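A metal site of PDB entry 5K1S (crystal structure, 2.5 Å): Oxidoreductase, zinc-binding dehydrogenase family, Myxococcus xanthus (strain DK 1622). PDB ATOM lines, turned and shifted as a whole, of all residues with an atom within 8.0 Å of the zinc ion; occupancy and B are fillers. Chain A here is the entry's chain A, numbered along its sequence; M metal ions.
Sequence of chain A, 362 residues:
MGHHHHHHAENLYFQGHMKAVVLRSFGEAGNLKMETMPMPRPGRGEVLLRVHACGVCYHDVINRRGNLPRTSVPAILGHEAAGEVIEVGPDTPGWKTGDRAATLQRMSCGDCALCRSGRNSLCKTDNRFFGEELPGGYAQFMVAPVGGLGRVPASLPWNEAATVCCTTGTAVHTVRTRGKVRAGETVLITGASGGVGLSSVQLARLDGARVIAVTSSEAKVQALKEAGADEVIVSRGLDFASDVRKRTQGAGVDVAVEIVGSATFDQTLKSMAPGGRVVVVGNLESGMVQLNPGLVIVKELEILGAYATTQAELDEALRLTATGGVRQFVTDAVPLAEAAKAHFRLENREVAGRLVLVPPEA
NH2 of Arg 106 is in hydrogen-bond range of O of Cys 123 (2.8 Å).
N of Gly 110 lies close to SG of Cys 115, 3.1 Å away.
The side-chain sulfur of Cys 123 lies close to the side-chain hydroxyl of Thr 125 (3.3 Å).
SG of Cys 123 lies close to N of Asp 126 (3.5 Å).
The side-chain hydroxyl (OG1) of Thr 125 lies close to the side-chain sulfur (SG) of Cys 109, at 2.8 Å.
The side-chain sulfur (SG) of Cys 112 lies close to the backbone NH (N) of Leu 114, at 3.7 Å.
The backbone carbonyl oxygen (O) of Cys 115 sits close to the side-chain amide oxygen (OD1) of Asn 120, at 3.4 Å.
The side-chain sulfur (SG) of Cys 109 lies close to the backbone NH (N) of Asp 111, at 3.3 Å.
Residues that only touch the zinc ion: Thr 125 and Gly 110.
Six residues have an atom within 4 Å of the zinc ion: Cys 109, Gly 110, Cys 112, Cys 115, Cys 123 and Thr 125.
The side-chain sulfur (SG) of Cys 115 binds the zinc ion (2.2 Å).
SG of Cys 112 binds the zinc ion, at 2.3 Å.
SG of Cys 109 binds the zinc ion (2.3 Å).
SG of Cys 123 binds the zinc ion (2.4 Å).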
ATOM      1  N   ARG A 106       6.363 -11.728  29.765  1.00  0.00           N
ATOM      2  CA  ARG A 106       7.587 -11.154  29.246  1.00  0.00           C
ATOM      3  C   ARG A 106       7.989 -11.878  27.970  1.00  0.00           C
ATOM      4  O   ARG A 106       7.505 -12.970  27.665  1.00  0.00           O
ATOM      5  CB  ARG A 106       8.727 -11.229  30.277  1.00  0.00           C
ATOM      6  CG  ARG A 106       9.062 -12.652  30.699  1.00  0.00           C
ATOM      7  CD  ARG A 106      10.224 -12.698  31.680  1.00  0.00           C
ATOM      8  NE  ARG A 106      11.492 -12.329  31.052  1.00  0.00           N
ATOM      9  CZ  ARG A 106      12.205 -13.128  30.266  1.00  0.00           C
ATOM     10  NH1 ARG A 106      11.774 -14.350  29.995  1.00  0.00           N
ATOM     11  NH2 ARG A 106      13.349 -12.705  29.752  1.00  0.00           N
ATOM     12  N   MET A 107       8.921 -11.262  27.239  1.00  0.00           N
ATOM     13  CA  MET A 107       9.408 -11.822  25.997  1.00  0.00           C
ATOM     14  C   MET A 107      10.611 -12.731  26.259  1.00  0.00           C
ATOM     15  O   MET A 107      11.054 -12.917  27.389  1.00  0.00           O
ATOM     16  CB  MET A 107       9.787 -10.700  25.019  1.00  0.00           C
ATOM     17  CG  MET A 107       8.600 -10.023  24.354  1.00  0.00           C
ATOM     18  SD  MET A 107       7.545 -11.184  23.478  1.00  0.00           S
ATOM     19  CE  MET A 107       8.693 -11.877  22.290  1.00  0.00           C
ATOM     20  N   SER A 108      11.144 -13.290  25.176  1.00  0.00           N
ATOM     21  CA  SER A 108      12.289 -14.200  25.240  1.00  0.00           C
ATOM     22  C   SER A 108      12.897 -14.263  23.847  1.00  0.00           C
ATOM     23  O   SER A 108      12.180 -14.463  22.869  1.00  0.00           O
ATOM     24  CB  SER A 108      11.859 -15.590  25.719  1.00  0.00           C
ATOM     25  OG  SER A 108      12.953 -16.487  25.746  1.00  0.00           O
ATOM     26  N   CYS A 109      14.222 -14.084  23.764  1.00  0.00           N
ATOM     27  CA  CYS A 109      14.860 -13.965  22.457  1.00  0.00           C
ATOM     28  C   CYS A 109      14.714 -15.249  21.653  1.00  0.00           C
ATOM     29  O   CYS A 109      14.374 -15.223  20.466  1.00  0.00           O
ATOM     30  CB  CYS A 109      16.325 -13.591  22.623  1.00  0.00           C
ATOM     31  SG  CYS A 109      17.409 -14.932  23.175  1.00  0.00           S
ATOM     32  N   GLY A 110      14.966 -16.391  22.281  1.00  0.00           N
ATOM     33  CA  GLY A 110      14.839 -17.679  21.626  1.00  0.00           C
ATOM     34  C   GLY A 110      16.123 -18.236  21.047  1.00  0.00           C
ATOM     35  O   GLY A 110      16.095 -19.342  20.484  1.00  0.00           O
ATOM     36  N   ASP A 111      17.240 -17.523  21.158  1.00  0.00           N
ATOM     37  CA  ASP A 111      18.497 -17.917  20.538  1.00  0.00           C
ATOM     38  C   ASP A 111      19.614 -18.207  21.521  1.00  0.00           C
ATOM     39  O   ASP A 111      20.501 -18.995  21.205  1.00  0.00           O
ATOM     40  CB  ASP A 111      18.965 -16.826  19.565  1.00  0.00           C
ATOM     41  CG  ASP A 111      17.991 -16.601  18.429  1.00  0.00           C
ATOM     42  OD1 ASP A 111      17.358 -17.585  17.980  1.00  0.00           O
ATOM     43  OD2 ASP A 111      17.847 -15.436  17.984  1.00  0.00           O
ATOM     44  N   CYS A 112      19.605 -17.582  22.697  1.00  0.00           N
ATOM     45  CA  CYS A 112      20.662 -17.821  23.669  1.00  0.00           C
ATOM     46  C   CYS A 112      20.562 -19.238  24.232  1.00  0.00           C
ATOM     47  O   CYS A 112      19.553 -19.921  24.092  1.00  0.00           O
ATOM     48  CB  CYS A 112      20.589 -16.793  24.803  1.00  0.00           C
ATOM     49  SG  CYS A 112      19.159 -16.989  25.896  1.00  0.00           S
ATOM     50  N   ALA A 113      21.653 -19.665  24.873  1.00  0.00           N
ATOM     51  CA  ALA A 113      21.698 -21.019  25.438  1.00  0.00           C
ATOM     52  C   ALA A 113      20.472 -21.297  26.304  1.00  0.00           C
ATOM     53  O   ALA A 113      19.831 -22.344  26.173  1.00  0.00           O
ATOM     54  CB  ALA A 113      22.981 -21.187  26.246  1.00  0.00           C
ATOM     55  N   LEU A 114      20.135 -20.364  27.191  1.00  0.00           N
ATOM     56  CA  LEU A 114      19.014 -20.569  28.107  1.00  0.00           C
ATOM     57  C   LEU A 114      17.728 -20.825  27.340  1.00  0.00           C
ATOM     58  O   LEU A 114      16.983 -21.761  27.655  1.00  0.00           O
ATOM     59  CB  LEU A 114      18.872 -19.371  29.037  1.00  0.00           C
ATOM     60  CG  LEU A 114      20.026 -19.151  29.999  1.00  0.00           C
ATOM     61  CD1 LEU A 114      20.013 -17.732  30.545  1.00  0.00           C
ATOM     62  CD2 LEU A 114      19.955 -20.156  31.145  1.00  0.00           C
ATOM     63  N   CYS A 115      17.439 -19.997  26.340  1.00  0.00           N
ATOM     64  CA  CYS A 115      16.243 -20.202  25.525  1.00  0.00           C
ATOM     65  C   CYS A 115      16.280 -21.552  24.830  1.00  0.00           C
ATOM     66  O   CYS A 115      15.292 -22.301  24.831  1.00  0.00           O
ATOM     67  CB  CYS A 115      16.108 -19.076  24.499  1.00  0.00           C
ATOM     68  SG  CYS A 115      15.481 -17.506  25.167  1.00  0.00           S
ATOM     69  N   ARG A 116      17.428 -21.893  24.219  1.00  0.00           N
ATOM     70  CA  ARG A 116      17.547 -23.175  23.540  1.00  0.00           C
ATOM     71  C   ARG A 116      17.376 -24.347  24.491  1.00  0.00           C
ATOM     72  O   ARG A 116      17.110 -25.472  24.039  1.00  0.00           O
ATOM     73  CB  ARG A 116      18.902 -23.278  22.829  1.00  0.00           C
ATOM     74  CG  ARG A 116      19.172 -22.168  21.810  1.00  0.00           C
ATOM     75  CD  ARG A 116      20.301 -22.535  20.858  1.00  0.00           C
ATOM     76  NE  ARG A 116      21.524 -22.908  21.553  1.00  0.00           N
ATOM     77  CZ  ARG A 116      22.483 -22.058  21.926  1.00  0.00           C
ATOM     78  NH1 ARG A 116      23.561 -22.507  22.555  1.00  0.00           N
ATOM     79  NH2 ARG A 116      22.360 -20.754  21.681  1.00  0.00           N
ATOM     80  N   ARG A 119      14.668 -22.754  29.063  1.00  0.00           N
ATOM     81  CA  ARG A 119      14.677 -21.866  30.232  1.00  0.00           C
ATOM     82  C   ARG A 119      14.376 -20.426  29.826  1.00  0.00           C
ATOM     83  O   ARG A 119      15.079 -19.502  30.218  1.00  0.00           O
ATOM     84  CB  ARG A 119      16.014 -21.962  30.956  1.00  0.00           C
ATOM     85  CG  ARG A 119      16.522 -23.380  31.173  1.00  0.00           C
ATOM     86  CD  ARG A 119      15.570 -24.195  32.040  1.00  0.00           C
ATOM     87  NE  ARG A 119      15.399 -23.615  33.359  1.00  0.00           N
ATOM     88  CZ  ARG A 119      16.213 -23.824  34.390  1.00  0.00           C
ATOM     89  NH1 ARG A 119      15.964 -23.250  35.565  1.00  0.00           N
ATOM     90  NH2 ARG A 119      17.291 -24.585  34.256  1.00  0.00           N
ATOM     91  N   ASN A 120      13.321 -20.243  29.033  1.00  0.00           N
ATOM     92  CA  ASN A 120      13.002 -18.904  28.526  1.00  0.00           C
ATOM     93  C   ASN A 120      12.777 -17.912  29.664  1.00  0.00           C
ATOM     94  O   ASN A 120      13.060 -16.717  29.504  1.00  0.00           O
ATOM     95  CB  ASN A 120      11.766 -18.970  27.626  1.00  0.00           C
ATOM     96  CG  ASN A 120      11.954 -19.926  26.460  1.00  0.00           C
ATOM     97  OD1 ASN A 120      12.718 -20.885  26.547  1.00  0.00           O
ATOM     98  ND2 ASN A 120      11.246 -19.667  25.364  1.00  0.00           N
ATOM     99  N   SER A 121      12.262 -18.377  30.809  1.00  0.00           N
ATOM    100  CA  SER A 121      12.070 -17.486  31.948  1.00  0.00           C
ATOM    101  C   SER A 121      13.356 -16.793  32.361  1.00  0.00           C
ATOM    102  O   SER A 121      13.297 -15.722  32.958  1.00  0.00           O
ATOM    103  CB  SER A 121      11.504 -18.280  33.130  1.00  0.00           C
ATOM    104  OG  SER A 121      10.241 -18.840  32.818  1.00  0.00           O
ATOM    105  N   LEU A 122      14.515 -17.385  32.041  1.00  0.00           N
ATOM    106  CA  LEU A 122      15.805 -16.867  32.474  1.00  0.00           C
ATOM    107  C   LEU A 122      16.537 -16.094  31.385  1.00  0.00           C
ATOM    108  O   LEU A 122      17.672 -15.658  31.614  1.00  0.00           O
ATOM    109  CB  LEU A 122      16.686 -18.016  32.960  1.00  0.00           C
ATOM    110  CG  LEU A 122      16.065 -18.911  34.034  1.00  0.00           C
ATOM    111  CD1 LEU A 122      17.000 -20.071  34.369  1.00  0.00           C
ATOM    112  CD2 LEU A 122      15.734 -18.119  35.288  1.00  0.00           C
ATOM    113  N   CYS A 123      15.925 -15.907  30.223  1.00  0.00           N
ATOM    114  CA  CYS A 123      16.585 -15.189  29.133  1.00  0.00           C
ATOM    115  C   CYS A 123      16.945 -13.778  29.563  1.00  0.00           C
ATOM    116  O   CYS A 123      16.119 -13.060  30.127  1.00  0.00           O
ATOM    117  CB  CYS A 123      15.680 -15.150  27.906  1.00  0.00           C
ATOM    118  SG  CYS A 123      16.344 -14.174  26.528  1.00  0.00           S
ATOM    119  N   LYS A 124      18.194 -13.376  29.289  1.00  0.00           N
ATOM    120  CA  LYS A 124      18.659 -12.035  29.606  1.00  0.00           C
ATOM    121  C   LYS A 124      18.714 -11.120  28.390  1.00  0.00           C
ATOM    122  O   LYS A 124      18.755  -9.890  28.562  1.00  0.00           O
ATOM    123  CB  LYS A 124      20.045 -12.078  30.252  1.00  0.00           C
ATOM    124  CG  LYS A 124      20.063 -12.605  31.684  1.00  0.00           C
ATOM    125  CD  LYS A 124      21.463 -12.553  32.267  1.00  0.00           C
ATOM    126  CE  LYS A 124      21.464 -12.883  33.757  1.00  0.00           C
ATOM    127  NZ  LYS A 124      22.844 -12.894  34.331  1.00  0.00           N
ATOM    128  N   THR A 125      18.714 -11.666  27.176  1.00  0.00           N
ATOM    129  CA  THR A 125      18.873 -10.835  25.983  1.00  0.00           C
ATOM    130  C   THR A 125      17.579 -10.138  25.589  1.00  0.00           C
ATOM    131  O   THR A 125      17.636  -9.069  24.965  1.00  0.00           O
ATOM    132  CB  THR A 125      19.382 -11.689  24.817  1.00  0.00           C
ATOM    133  OG1 THR A 125      18.408 -12.696  24.490  1.00  0.00           O
ATOM    134  CG2 THR A 125      20.695 -12.372  25.178  1.00  0.00           C
ATOM    135  N   ASP A 126      16.432 -10.707  25.931  1.00  0.00           N
ATOM    136  CA  ASP A 126      15.130 -10.065  25.676  1.00  0.00           C
ATOM    137  C   ASP A 126      14.260 -10.291  26.905  1.00  0.00           C
ATOM    138  O   ASP A 126      13.667 -11.367  27.061  1.00  0.00           O
ATOM    139  CB  ASP A 126      14.469 -10.610  24.419  1.00  0.00           C
ATOM    140  CG  ASP A 126      13.209  -9.857  24.053  1.00  0.00           C
ATOM    141  OD1 ASP A 126      12.711  -9.069  24.887  1.00  0.00           O
ATOM    142  OD2 ASP A 126      12.689 -10.059  22.930  1.00  0.00           O
ATOM    143  N   ASN A 127      14.191  -9.290  27.777  1.00  0.00           N
ATOM    144  CA  ASN A 127      13.381  -9.360  28.998  1.00  0.00           C
ATOM    145  C   ASN A 127      12.243  -8.342  28.981  1.00  0.00           C
ATOM    146  O   ASN A 127      11.766  -7.945  30.050  1.00  0.00           O
ATOM    147  CB  ASN A 127      14.264  -9.153  30.228  1.00  0.00           C
ATOM    148  CG  ASN A 127      15.056  -7.860  30.170  1.00  0.00           C
ATOM    149  OD1 ASN A 127      14.824  -7.013  29.298  1.00  0.00           O
ATOM    150  ND2 ASN A 127      15.986  -7.685  31.101  1.00  0.00           N
HETATM  151 ZN    ZN M   1      17.160 -16.051  25.196  1.00  0.00          ZN
